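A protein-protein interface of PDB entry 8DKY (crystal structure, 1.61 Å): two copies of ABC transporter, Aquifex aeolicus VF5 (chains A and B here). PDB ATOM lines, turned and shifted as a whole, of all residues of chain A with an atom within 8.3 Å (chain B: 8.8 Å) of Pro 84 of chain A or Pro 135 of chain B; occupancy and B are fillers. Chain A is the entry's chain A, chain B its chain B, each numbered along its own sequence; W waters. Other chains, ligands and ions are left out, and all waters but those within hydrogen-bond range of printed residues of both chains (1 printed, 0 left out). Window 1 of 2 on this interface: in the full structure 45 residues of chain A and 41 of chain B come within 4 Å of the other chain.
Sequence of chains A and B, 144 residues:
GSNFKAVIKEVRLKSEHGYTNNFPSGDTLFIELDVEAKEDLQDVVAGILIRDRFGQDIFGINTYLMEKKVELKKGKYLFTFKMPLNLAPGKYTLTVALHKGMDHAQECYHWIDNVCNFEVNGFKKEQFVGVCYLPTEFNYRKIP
The backbone carbonyl oxygen of Lys 82 of chain A lies within hydrogen-bond range of the backbone NH of Glu 137 of chain B (2.9 Å).
O of Leu 87 of chain A is in hydrogen-bond range of OG of Ser 25 of chain A. O of Asn 86 of chain B sits at hydrogen-bond distance from N of Tyr 133 of chain B, at 3.0 Å. The backbone NH of Ile 50 of chain A sits at hydrogen-bond distance from the backbone carbonyl oxygen of Phe 59 of chain A (2.8 Å). N of Leu 29 of chain A lies within hydrogen-bond range of O of Met 83 of chain A (2.8 Å). The backbone carbonyl oxygen of Asn 86 of chain A is in hydrogen-bond range of the backbone NH of Tyr 133 of chain A, 3.0 Å away. The side-chain hydroxyl of Thr 136 of chain B is in hydrogen-bond range of the backbone carbonyl oxygen of Leu 134 of chain B, 2.8 Å away.
Among the printed residues, merely in contact across the chains: Phe 59 of chain A with Phe 128 of chain B (3.8 Å), Phe 59 of chain A with Cys 132 of chain B (3.1 Å), Phe 59 of chain A with Tyr 133 of chain B (3.9 Å), Phe 59 of chain A with Leu 134 of chain B (3.4 Å), Phe 59 of chain A with Thr 136 of chain B (3.5 Å), Ile 61 of chain A with Glu 126 of chain B (3.9 Å), Met 66 of chain A with Thr 136 of chain B (3.6 Å), Met 66 of chain A with Glu 137 of chain B (3.9 Å), Met 66 of chain A with Phe 138 of chain B (3.5 Å), Phe 81 of chain A with Thr 136 of chain B (3.8 Å), Phe 81 of chain A with Glu 137 of chain B (3.2 Å), Phe 81 of chain A with Phe 138 of chain B (3.5 Å), Lys 82 of chain A with Pro 135 of chain B (3.7 Å), Lys 82 of chain A with Thr 136 of chain B (3.2 Å), Met 83 of chain A with Leu 134 of chain B (3.9 Å), Met 83 of chain A with Pro 135 of chain B (3.5 Å), Met 83 of chain A with Thr 136 of chain B (3.7 Å), Pro 84 of chain A with Leu 134 of chain B (3.4 Å), Pro 84 of chain A with Pro 135 of chain B (3.1 Å), Asn 86 of chain A with Leu 134 of chain B (3.8 Å), Leu 87 of chain A with Cys 132 of chain B (3.7 Å) and Pro 135 of chain A with Pro 84 of chain B (3.1 Å).
Pro 84 of chain A touches just these residues of chain B: Leu 134 and Pro 135. Pro 135 of chain B touches just these residues of chain A: Lys 82, Met 83 and Pro 84. Of the printed residues of chain A, Leu 134 of chain B touches Phe 59 (3.4 Å), Met 83 (3.9 Å), Pro 84 (3.4 Å) and Asn 86 (3.8 Å). Printed residues of chain B within 4 Å of Met 83 of chain A: Leu 134, Pro 135 and Thr 136. Printed residues of chain B within 4 Å of Leu 87 of chain A: Cys 132. Of the printed residues of chain A, Pro 84 of chain B touches Pro 135 (3.1 Å). Of the printed residues of chain B, Phe 81 of chain A touches Thr 136, Glu 137 and Phe 138. Leu 85 of chain A touches none of the printed residues of chain B. The nearest residue of chain B that does not touch Pro 84 of chain A is Thr 136 of chain B (5.3 Å). The nearest residue of chain A that does not touch Pro 135 of chain B is Asn 86 of chain A (4.9 Å). The nearest printed residue of chain B that does not touch Pro 135 of chain A is Asn 86 of chain B (5.0 Å).
Of the 12 printed residues of chain B, 10 touch a printed residue of chain A. Hydrophobic or aromatic side chains of chain B within 4 Å of the printed part of chain A: Pro 84, Phe 128, Leu 134, Pro 135 and Phe 138. Of the 21 printed residues of chain A, 10 touch a printed residue of chain B. Hydrophobic or aromatic side chains of chain A within 4 Å of the printed part of chain B: Phe 59, Ile 61, Met 66, Phe 81, Met 83, Pro 84, Leu 87 and Pro 135. Among the printed residues, no Asp or Glu carboxylate lies within 4 Å of a Lys or Arg side-chain nitrogen of the other chain.
Pro 84 of chain A touches Pro 135 of chain B, and with the chains exchanged Pro 135 of chain A touches Pro 84 of chain B. Positions printed for both chains: 84, 86, 125, 133 and 135. Of the 23 pairs that touch across the chains among the printed residues, 2 have their exchanged pair printed and touching as well.
Water W1 lies within hydrogen-bond range of the backbone carbonyl oxygen (O) of Tyr 133 of chain A (3.1 Å), the side-chain amide nitrogen (ND2) of Asn 86 of chain B (3.2 Å), the backbone carbonyl oxygen (O) of Tyr 133 of chain B (3.4 Å) and the side-chain amide nitrogen (ND2) of Asn 86 of chain A (3.5 Å).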
ATOM      1  N   PRO A  24      -8.274  -5.779 -12.295  1.00  0.00           N
ATOM      2  CA  PRO A  24      -6.943  -5.848 -12.895  1.00  0.00           C
ATOM      3  C   PRO A  24      -6.735  -4.654 -13.808  1.00  0.00           C
ATOM      4  O   PRO A  24      -7.668  -4.159 -14.445  1.00  0.00           O
ATOM      5  CB  PRO A  24      -6.971  -7.158 -13.691  1.00  0.00           C
ATOM      6  CG  PRO A  24      -8.405  -7.388 -13.984  1.00  0.00           C
ATOM      7  CD  PRO A  24      -9.188  -6.795 -12.844  1.00  0.00           C
ATOM      8  N   SER A  25      -5.496  -4.176 -13.848  1.00  0.00           N
ATOM      9  CA  SER A  25      -5.185  -3.012 -14.665  1.00  0.00           C
ATOM     10  C   SER A  25      -5.607  -3.254 -16.107  1.00  0.00           C
ATOM     11  O   SER A  25      -5.292  -4.294 -16.692  1.00  0.00           O
ATOM     12  CB  SER A  25      -3.690  -2.698 -14.583  1.00  0.00           C
ATOM     13  OG  SER A  25      -3.384  -1.518 -15.308  1.00  0.00           O
ATOM     14  N   GLY A  26      -6.312  -2.281 -16.682  1.00  0.00           N
ATOM     15  CA  GLY A  26      -6.802  -2.380 -18.039  1.00  0.00           C
ATOM     16  C   GLY A  26      -8.225  -2.881 -18.161  1.00  0.00           C
ATOM     17  O   GLY A  26      -8.796  -2.813 -19.258  1.00  0.00           O
ATOM     18  N   ASP A  27      -8.808  -3.383 -17.076  1.00  0.00           N
ATOM     19  CA  ASP A  27     -10.197  -3.813 -17.093  1.00  0.00           C
ATOM     20  C   ASP A  27     -11.125  -2.630 -17.335  1.00  0.00           C
ATOM     21  O   ASP A  27     -10.801  -1.480 -17.025  1.00  0.00           O
ATOM     22  CB  ASP A  27     -10.566  -4.492 -15.772  1.00  0.00           C
ATOM     23  CG  ASP A  27     -11.711  -5.475 -15.922  1.00  0.00           C
ATOM     24  OD1 ASP A  27     -12.085  -5.787 -17.072  1.00  0.00           O
ATOM     25  OD2 ASP A  27     -12.241  -5.933 -14.887  1.00  0.00           O
ATOM     26  N   THR A  28     -12.293  -2.926 -17.895  1.00  0.00           N
ATOM     27  CA  THR A  28     -13.300  -1.901 -18.121  1.00  0.00           C
ATOM     28  C   THR A  28     -14.054  -1.623 -16.827  1.00  0.00           C
ATOM     29  O   THR A  28     -14.568  -2.544 -16.184  1.00  0.00           O
ATOM     30  CB  THR A  28     -14.273  -2.330 -19.220  1.00  0.00           C
ATOM     31  OG1 THR A  28     -13.571  -2.440 -20.465  1.00  0.00           O
ATOM     32  CG2 THR A  28     -15.391  -1.309 -19.366  1.00  0.00           C
ATOM     33  N   LEU A  29     -14.102  -0.353 -16.443  1.00  0.00           N
ATOM     34  CA  LEU A  29     -14.821   0.104 -15.266  1.00  0.00           C
ATOM     35  C   LEU A  29     -16.111   0.790 -15.692  1.00  0.00           C
ATOM     36  O   LEU A  29     -16.099   1.664 -16.571  1.00  0.00           O
ATOM     37  CB  LEU A  29     -13.960   1.069 -14.449  1.00  0.00           C
ATOM     38  CG  LEU A  29     -14.647   1.876 -13.343  1.00  0.00           C
ATOM     39  CD1 LEU A  29     -15.297   0.973 -12.312  1.00  0.00           C
ATOM     40  CD2 LEU A  29     -13.658   2.823 -12.677  1.00  0.00           C
ATOM     41  N   PHE A  30     -17.217   0.373 -15.081  1.00  0.00           N
ATOM     42  CA  PHE A  30     -18.487   1.075 -15.151  1.00  0.00           C
ATOM     43  C   PHE A  30     -18.743   1.749 -13.812  1.00  0.00           C
ATOM     44  O   PHE A  30     -18.548   1.144 -12.752  1.00  0.00           O
ATOM     45  CB  PHE A  30     -19.651   0.134 -15.471  1.00  0.00           C
ATOM     46  CG  PHE A  30     -19.502  -0.608 -16.764  1.00  0.00           C
ATOM     47  CD1 PHE A  30     -20.147  -0.166 -17.905  1.00  0.00           C
ATOM     48  CD2 PHE A  30     -18.744  -1.765 -16.831  1.00  0.00           C
ATOM     49  CE1 PHE A  30     -20.021  -0.851 -19.097  1.00  0.00           C
ATOM     50  CE2 PHE A  30     -18.614  -2.456 -18.019  1.00  0.00           C
ATOM     51  CZ  PHE A  30     -19.253  -1.998 -19.154  1.00  0.00           C
ATOM     52  N   ILE A  50     -10.943  10.477 -10.344  1.00  0.00           N
ATOM     53  CA  ILE A  50     -10.152   9.422  -9.724  1.00  0.00           C
ATOM     54  C   ILE A  50      -8.882  10.034  -9.158  1.00  0.00           C
ATOM     55  O   ILE A  50      -8.124  10.696  -9.887  1.00  0.00           O
ATOM     56  CB  ILE A  50      -9.805   8.324 -10.743  1.00  0.00           C
ATOM     57  CG1 ILE A  50     -11.064   7.633 -11.261  1.00  0.00           C
ATOM     58  CG2 ILE A  50      -8.832   7.319 -10.137  1.00  0.00           C
ATOM     59  CD1 ILE A  50     -10.804   6.768 -12.481  1.00  0.00           C
ATOM     60  N   PHE A  59      -7.292  11.096 -12.785  1.00  0.00           N
ATOM     61  CA  PHE A  59      -8.068  11.359 -13.997  1.00  0.00           C
ATOM     62  C   PHE A  59      -9.454  11.865 -13.642  1.00  0.00           C
ATOM     63  O   PHE A  59     -10.193  11.181 -12.939  1.00  0.00           O
ATOM     64  CB  PHE A  59      -8.209  10.112 -14.875  1.00  0.00           C
ATOM     65  CG  PHE A  59      -9.238  10.264 -15.961  1.00  0.00           C
ATOM     66  CD1 PHE A  59      -9.021  11.127 -17.026  1.00  0.00           C
ATOM     67  CD2 PHE A  59     -10.444   9.581 -15.895  1.00  0.00           C
ATOM     68  CE1 PHE A  59      -9.972  11.279 -18.021  1.00  0.00           C
ATOM     69  CE2 PHE A  59     -11.401   9.732 -16.885  1.00  0.00           C
ATOM     70  CZ  PHE A  59     -11.165  10.581 -17.949  1.00  0.00           C
ATOM     71  N   ILE A  61     -13.037  13.989 -15.384  1.00  0.00           N
ATOM     72  CA  ILE A  61     -13.730  14.459 -16.581  1.00  0.00           C
ATOM     73  C   ILE A  61     -15.196  14.649 -16.223  1.00  0.00           C
ATOM     74  O   ILE A  61     -15.684  14.102 -15.232  1.00  0.00           O
ATOM     75  CB  ILE A  61     -13.545  13.465 -17.758  1.00  0.00           C
ATOM     76  CG1 ILE A  61     -13.827  14.133 -19.108  1.00  0.00           C
ATOM     77  CG2 ILE A  61     -14.429  12.233 -17.569  1.00  0.00           C
ATOM     78  CD1 ILE A  61     -13.409  13.287 -20.307  1.00  0.00           C
ATOM     79  N   MET A  66     -17.161  16.242 -22.274  1.00  0.00           N
ATOM     80  CA  MET A  66     -17.473  15.187 -23.226  1.00  0.00           C
ATOM     81  C   MET A  66     -18.527  15.619 -24.239  1.00  0.00           C
ATOM     82  O   MET A  66     -18.935  14.815 -25.079  1.00  0.00           O
ATOM     83  CB  MET A  66     -17.945  13.934 -22.491  1.00  0.00           C
ATOM     84  CG  MET A  66     -16.900  13.370 -21.542  1.00  0.00           C
ATOM     85  SD  MET A  66     -17.606  12.234 -20.332  1.00  0.00           S
ATOM     86  CE  MET A  66     -18.224  10.955 -21.417  1.00  0.00           C
ATOM     87  N   PHE A  81     -21.032   5.815 -16.440  1.00  0.00           N
ATOM     88  CA  PHE A  81     -19.762   6.096 -17.092  1.00  0.00           C
ATOM     89  C   PHE A  81     -19.045   4.782 -17.382  1.00  0.00           C
ATOM     90  O   PHE A  81     -19.185   3.811 -16.636  1.00  0.00           O
ATOM     91  CB  PHE A  81     -18.859   6.969 -16.212  1.00  0.00           C
ATOM     92  CG  PHE A  81     -19.311   8.394 -16.084  1.00  0.00           C
ATOM     93  CD1 PHE A  81     -18.797   9.373 -16.918  1.00  0.00           C
ATOM     94  CD2 PHE A  81     -20.217   8.760 -15.104  1.00  0.00           C
ATOM     95  CE1 PHE A  81     -19.199  10.688 -16.791  1.00  0.00           C
ATOM     96  CE2 PHE A  81     -20.623  10.075 -14.973  1.00  0.00           C
ATOM     97  CZ  PHE A  81     -20.115  11.039 -15.816  1.00  0.00           C
ATOM     98  N   LYS A  82     -18.256   4.761 -18.455  1.00  0.00           N
ATOM     99  CA  LYS A  82     -17.501   3.572 -18.832  1.00  0.00           C
ATOM    100  C   LYS A  82     -16.117   3.984 -19.311  1.00  0.00           C
ATOM    101  O   LYS A  82     -15.985   4.949 -20.066  1.00  0.00           O
ATOM    102  CB  LYS A  82     -18.228   2.782 -19.928  1.00  0.00           C
ATOM    103  CG  LYS A  82     -17.482   1.556 -20.437  1.00  0.00           C
ATOM    104  CD  LYS A  82     -18.188   0.976 -21.655  1.00  0.00           C
ATOM    105  CE  LYS A  82     -17.500  -0.278 -22.164  1.00  0.00           C
ATOM    106  NZ  LYS A  82     -18.234  -0.876 -23.313  1.00  0.00           N
ATOM    107  N   MET A  83     -15.088   3.252 -18.876  1.00  0.00           N
ATOM    108  CA  MET A  83     -13.721   3.651 -19.198  1.00  0.00           C
ATOM    109  C   MET A  83     -12.768   2.489 -18.957  1.00  0.00           C
ATOM    110  O   MET A  83     -12.981   1.702 -18.032  1.00  0.00           O
ATOM    111  CB  MET A  83     -13.313   4.872 -18.361  1.00  0.00           C
ATOM    112  CG  MET A  83     -12.820   4.557 -16.958  1.00  0.00           C
ATOM    113  SD  MET A  83     -12.992   6.016 -15.920  1.00  0.00           S
ATOM    114  CE  MET A  83     -14.743   6.299 -16.137  1.00  0.00           C
ATOM    115  N   PRO A  84     -11.718   2.348 -19.770  1.00  0.00           N
ATOM    116  CA  PRO A  84     -10.671   1.368 -19.449  1.00  0.00           C
ATOM    117  C   PRO A  84      -9.824   1.882 -18.297  1.00  0.00           C
ATOM    118  O   PRO A  84      -9.366   3.026 -18.308  1.00  0.00           O
ATOM    119  CB  PRO A  84      -9.858   1.269 -20.745  1.00  0.00           C
ATOM    120  CG  PRO A  84     -10.104   2.566 -21.429  1.00  0.00           C
ATOM    121  CD  PRO A  84     -11.534   2.916 -21.115  1.00  0.00           C
ATOM    122  N   LEU A  85      -9.619   1.032 -17.295  1.00  0.00           N
ATOM    123  CA  LEU A  85      -8.953   1.472 -16.073  1.00  0.00           C
ATOM    124  C   LEU A  85      -7.450   1.231 -16.237  1.00  0.00           C
ATOM    125  O   LEU A  85      -6.836   0.351 -15.628  1.00  0.00           O
ATOM    126  CB  LEU A  85      -9.561   0.765 -14.867  1.00  0.00           C
ATOM    127  CG  LEU A  85      -9.170   1.137 -13.442  1.00  0.00           C
ATOM    128  CD1 LEU A  85      -9.571   2.574 -13.176  1.00  0.00           C
ATOM    129  CD2 LEU A  85      -9.908   0.225 -12.483  1.00  0.00           C
ATOM    130  N   ASN A  86      -6.869   2.045 -17.125  1.00  0.00           N
ATOM    131  CA  ASN A  86      -5.472   1.924 -17.547  1.00  0.00           C
ATOM    132  C   ASN A  86      -4.550   2.619 -16.543  1.00  0.00           C
ATOM    133  O   ASN A  86      -3.852   3.587 -16.848  1.00  0.00           O
ATOM    134  CB  ASN A  86      -5.302   2.508 -18.945  1.00  0.00           C
ATOM    135  CG  ASN A  86      -6.002   1.687 -20.012  1.00  0.00           C
ATOM    136  OD1 ASN A  86      -6.243   0.496 -19.833  1.00  0.00           O
ATOM    137  ND2 ASN A  86      -6.349   2.330 -21.121  1.00  0.00           N
ATOM    138  N   LEU A  87      -4.562   2.101 -15.318  1.00  0.00           N
ATOM    139  CA  LEU A  87      -3.873   2.722 -14.199  1.00  0.00           C
ATOM    140  C   LEU A  87      -2.923   1.725 -13.554  1.00  0.00           C
ATOM    141  O   LEU A  87      -3.057   0.509 -13.717  1.00  0.00           O
ATOM    142  CB  LEU A  87      -4.865   3.236 -13.147  1.00  0.00           C
ATOM    143  CG  LEU A  87      -5.871   4.308 -13.570  1.00  0.00           C
ATOM    144  CD1 LEU A  87      -6.729   4.728 -12.384  1.00  0.00           C
ATOM    145  CD2 LEU A  87      -5.174   5.509 -14.186  1.00  0.00           C
ATOM    146  N   LYS A 125      -3.324  -7.243 -18.861  1.00  0.00           N
ATOM    147  CA  LYS A 125      -2.622  -7.265 -20.124  1.00  0.00           C
ATOM    148  C   LYS A 125      -1.135  -7.386 -19.838  1.00  0.00           C
ATOM    149  O   LYS A 125      -0.715  -8.165 -18.961  1.00  0.00           O
ATOM    150  CB  LYS A 125      -2.905  -5.986 -20.929  1.00  0.00           C
ATOM    151  CG  LYS A 125      -4.379  -5.694 -21.173  1.00  0.00           C
ATOM    152  CD  LYS A 125      -4.596  -4.415 -21.949  1.00  0.00           C
ATOM    153  CE  LYS A 125      -6.058  -4.284 -22.326  1.00  0.00           C
ATOM    154  NZ  LYS A 125      -6.942  -4.660 -21.189  1.00  0.00           N
ATOM    155  N   TYR A 133      -1.074   3.291 -18.063  1.00  0.00           N
ATOM    156  CA  TYR A 133      -0.774   2.346 -19.129  1.00  0.00           C
ATOM    157  C   TYR A 133      -1.141   2.962 -20.468  1.00  0.00           C
ATOM    158  O   TYR A 133      -2.291   3.363 -20.674  1.00  0.00           O
ATOM    159  CB  TYR A 133      -1.550   1.049 -18.944  1.00  0.00           C
ATOM    160  CG  TYR A 133      -1.482   0.122 -20.135  1.00  0.00           C
ATOM    161  CD1 TYR A 133      -2.520   0.074 -21.064  1.00  0.00           C
ATOM    162  CD2 TYR A 133      -0.416  -0.755 -20.301  1.00  0.00           C
ATOM    163  CE1 TYR A 133      -2.482  -0.796 -22.136  1.00  0.00           C
ATOM    164  CE2 TYR A 133      -0.373  -1.631 -21.371  1.00  0.00           C
ATOM    165  CZ  TYR A 133      -1.408  -1.646 -22.286  1.00  0.00           C
ATOM    166  OH  TYR A 133      -1.370  -2.511 -23.357  1.00  0.00           O
ATOM    167  N   PRO A 135      -1.466   1.760 -24.292  1.00  0.00           N
ATOM    168  CA  PRO A 135      -1.416   0.588 -25.183  1.00  0.00           C
ATOM    169  C   PRO A 135      -0.366   0.777 -26.267  1.00  0.00           C
ATOM    170  O   PRO A 135      -0.426   1.725 -27.054  1.00  0.00           O
ATOM    171  CB  PRO A 135      -2.834   0.517 -25.764  1.00  0.00           C
ATOM    172  CG  PRO A 135      -3.490   1.829 -25.410  1.00  0.00           C
ATOM    173  CD  PRO A 135      -2.824   2.310 -24.167  1.00  0.00           C
ATOM    174  N   PRO B  84      -0.789   5.735 -28.006  1.00  0.00           N
ATOM    175  CA  PRO B  84      -1.525   6.991 -27.869  1.00  0.00           C
ATOM    176  C   PRO B  84      -1.015   7.721 -26.645  1.00  0.00           C
ATOM    177  O   PRO B  84      -0.775   7.118 -25.598  1.00  0.00           O
ATOM    178  CB  PRO B  84      -2.976   6.541 -27.691  1.00  0.00           C
ATOM    179  CG  PRO B  84      -2.849   5.223 -27.026  1.00  0.00           C
ATOM    180  CD  PRO B  84      -1.591   4.584 -27.563  1.00  0.00           C
ATOM    181  N   ASN B  86      -1.823   9.527 -24.095  1.00  0.00           N
ATOM    182  CA  ASN B  86      -2.940   9.884 -23.214  1.00  0.00           C
ATOM    183  C   ASN B  86      -2.431  10.413 -21.870  1.00  0.00           C
ATOM    184  O   ASN B  86      -2.694   9.862 -20.798  1.00  0.00           O
ATOM    185  CB  ASN B  86      -3.851   8.680 -23.003  1.00  0.00           C
ATOM    186  CG  ASN B  86      -4.490   8.193 -24.288  1.00  0.00           C
ATOM    187  OD1 ASN B  86      -4.652   8.954 -25.241  1.00  0.00           O
ATOM    188  ND2 ASN B  86      -4.859   6.918 -24.318  1.00  0.00           N
ATOM    189  N   LYS B 125      -8.386  14.969 -27.905  1.00  0.00           N
ATOM    190  CA  LYS B 125      -9.711  14.456 -27.595  1.00  0.00           C
ATOM    191  C   LYS B 125     -10.368  15.392 -26.592  1.00  0.00           C
ATOM    192  O   LYS B 125     -10.217  16.614 -26.691  1.00  0.00           O
ATOM    193  CB  LYS B 125      -9.609  13.025 -27.063  1.00  0.00           C
ATOM    194  CG  LYS B 125      -8.687  12.150 -27.909  1.00  0.00           C
ATOM    195  CD  LYS B 125      -8.899  10.668 -27.664  1.00  0.00           C
ATOM    196  CE  LYS B 125      -7.582   9.913 -27.771  1.00  0.00           C
ATOM    197  NZ  LYS B 125      -7.063   9.891 -29.169  1.00  0.00           N
ATOM    198  N   GLU B 126     -11.084  14.842 -25.619  1.00  0.00           N
ATOM    199  CA  GLU B 126     -11.710  15.681 -24.610  1.00  0.00           C
ATOM    200  C   GLU B 126     -10.664  16.300 -23.692  1.00  0.00           C
ATOM    201  O   GLU B 126      -9.579  15.751 -23.481  1.00  0.00           O
ATOM    202  CB  GLU B 126     -12.705  14.871 -23.779  1.00  0.00           C
ATOM    203  CG  GLU B 126     -13.815  14.235 -24.585  1.00  0.00           C
ATOM    204  CD  GLU B 126     -13.483  12.815 -24.986  1.00  0.00           C
ATOM    205  OE1 GLU B 126     -12.350  12.374 -24.705  1.00  0.00           O
ATOM    206  OE2 GLU B 126     -14.353  12.143 -25.576  1.00  0.00           O
ATOM    207  N   PHE B 128      -9.476  17.208 -19.908  1.00  0.00           N
ATOM    208  CA  PHE B 128      -9.546  16.389 -18.705  1.00  0.00           C
ATOM    209  C   PHE B 128      -8.554  16.925 -17.683  1.00  0.00           C
ATOM    210  O   PHE B 128      -7.634  17.674 -18.018  1.00  0.00           O
ATOM    211  CB  PHE B 128      -9.248  14.918 -19.017  1.00  0.00           C
ATOM    212  CG  PHE B 128      -7.824  14.666 -19.428  1.00  0.00           C
ATOM    213  CD1 PHE B 128      -6.878  14.289 -18.488  1.00  0.00           C
ATOM    214  CD2 PHE B 128      -7.423  14.846 -20.741  1.00  0.00           C
ATOM    215  CE1 PHE B 128      -5.566  14.068 -18.852  1.00  0.00           C
ATOM    216  CE2 PHE B 128      -6.106  14.627 -21.113  1.00  0.00           C
ATOM    217  CZ  PHE B 128      -5.179  14.237 -20.166  1.00  0.00           C
ATOM    218  N   CYS B 132      -3.387  11.538 -16.436  1.00  0.00           N
ATOM    219  CA  CYS B 132      -3.574  10.752 -17.643  1.00  0.00           C
ATOM    220  C   CYS B 132      -5.030  10.819 -18.072  1.00  0.00           C
ATOM    221  O   CYS B 132      -5.905  11.277 -17.332  1.00  0.00           O
ATOM    222  CB  CYS B 132      -3.140   9.297 -17.438  1.00  0.00           C
ATOM    223  SG  CYS B 132      -4.058   8.424 -16.147  1.00  0.00           S
ATOM    224  N   TYR B 133      -5.270  10.341 -19.288  1.00  0.00           N
ATOM    225  CA  TYR B 133      -6.577  10.363 -19.923  1.00  0.00           C
ATOM    226  C   TYR B 133      -7.061   8.935 -20.135  1.00  0.00           C
ATOM    227  O   TYR B 133      -6.332   8.104 -20.684  1.00  0.00           O
ATOM    228  CB  TYR B 133      -6.502  11.105 -21.259  1.00  0.00           C
ATOM    229  CG  TYR B 133      -7.691  10.901 -22.164  1.00  0.00           C
ATOM    230  CD1 TYR B 133      -8.896  11.552 -21.925  1.00  0.00           C
ATOM    231  CD2 TYR B 133      -7.610  10.055 -23.261  1.00  0.00           C
ATOM    232  CE1 TYR B 133      -9.983  11.366 -22.759  1.00  0.00           C
ATOM    233  CE2 TYR B 133      -8.688   9.861 -24.097  1.00  0.00           C
ATOM    234  CZ  TYR B 133      -9.872  10.518 -23.843  1.00  0.00           C
ATOM    235  OH  TYR B 133     -10.948  10.323 -24.678  1.00  0.00           O
ATOM    236  N   LEU B 134      -8.281   8.651 -19.686  1.00  0.00           N
ATOM    237  CA  LEU B 134      -8.941   7.389 -19.963  1.00  0.00           C
ATOM    238  C   LEU B 134     -10.120   7.637 -20.890  1.00  0.00           C
ATOM    239  O   LEU B 134     -10.983   8.462 -20.561  1.00  0.00           O
ATOM    240  CB  LEU B 134      -9.432   6.729 -18.666  1.00  0.00           C
ATOM    241  CG  LEU B 134      -8.444   6.502 -17.518  1.00  0.00           C
ATOM    242  CD1 LEU B 134      -9.141   5.813 -16.347  1.00  0.00           C
ATOM    243  CD2 LEU B 134      -7.242   5.689 -17.978  1.00  0.00           C
ATOM    244  N   PRO B 135     -10.198   6.968 -22.041  1.00  0.00           N
ATOM    245  CA  PRO B 135     -11.331   7.189 -22.956  1.00  0.00           C
ATOM    246  C   PRO B 135     -12.642   6.778 -22.300  1.00  0.00           C
ATOM    247  O   PRO B 135     -12.832   5.617 -21.933  1.00  0.00           O
ATOM    248  CB  PRO B 135     -10.994   6.305 -24.164  1.00  0.00           C
ATOM    249  CG  PRO B 135      -9.999   5.313 -23.652  1.00  0.00           C
ATOM    250  CD  PRO B 135      -9.212   6.027 -22.597  1.00  0.00           C
ATOM    251  N   THR B 136     -13.550   7.742 -22.156  1.00  0.00           N
ATOM    252  CA  THR B 136     -14.733   7.596 -21.319  1.00  0.00           C
ATOM    253  C   THR B 136     -16.002   7.767 -22.144  1.00  0.00           C
ATOM    254  O   THR B 136     -16.058   8.601 -23.055  1.00  0.00           O
ATOM    255  CB  THR B 136     -14.710   8.620 -20.173  1.00  0.00           C
ATOM    256  OG1 THR B 136     -13.515   8.446 -19.403  1.00  0.00           O
ATOM    257  CG2 THR B 136     -15.922   8.456 -19.259  1.00  0.00           C
ATOM    258  N   GLU B 137     -17.019   6.971 -21.813  1.00  0.00           N
ATOM    259  CA  GLU B 137     -18.334   7.053 -22.428  1.00  0.00           C
ATOM    260  C   GLU B 137     -19.383   7.244 -21.342  1.00  0.00           C
ATOM    261  O   GLU B 137     -19.179   6.857 -20.188  1.00  0.00           O
ATOM    262  CB  GLU B 137     -18.639   5.794 -23.247  1.00  0.00           C
ATOM    263  CG  GLU B 137     -17.546   5.438 -24.238  1.00  0.00           C
ATOM    264  CD  GLU B 137     -17.847   4.175 -25.012  1.00  0.00           C
ATOM    265  OE1 GLU B 137     -17.535   4.126 -26.221  1.00  0.00           O
ATOM    266  OE2 GLU B 137     -18.394   3.228 -24.409  1.00  0.00           O
ATOM    267  N   PHE B 138     -20.513   7.837 -21.723  1.00  0.00           N
ATOM    268  CA  PHE B 138     -21.545   8.231 -20.774  1.00  0.00           C
ATOM    269  C   PHE B 138     -22.929   8.026 -21.371  1.00  0.00           C
ATOM    270  O   PHE B 138     -23.136   8.223 -22.570  1.00  0.00           O
ATOM    271  CB  PHE B 138     -21.356   9.700 -20.351  1.00  0.00           C
ATOM    272  CG  PHE B 138     -22.499  10.267 -19.554  1.00  0.00           C
ATOM    273  CD1 PHE B 138     -22.508  10.184 -18.173  1.00  0.00           C
ATOM    274  CD2 PHE B 138     -23.538  10.935 -20.188  1.00  0.00           C
ATOM    275  CE1 PHE B 138     -23.550  10.718 -17.445  1.00  0.00           C
ATOM    276  CE2 PHE B 138     -24.581  11.469 -19.464  1.00  0.00           C
ATOM    277  CZ  PHE B 138     -24.586  11.365 -18.096  1.00  0.00           C
HETATM  278  O   HOH W   1      -4.588   5.319 -21.574  1.00  0.00           O
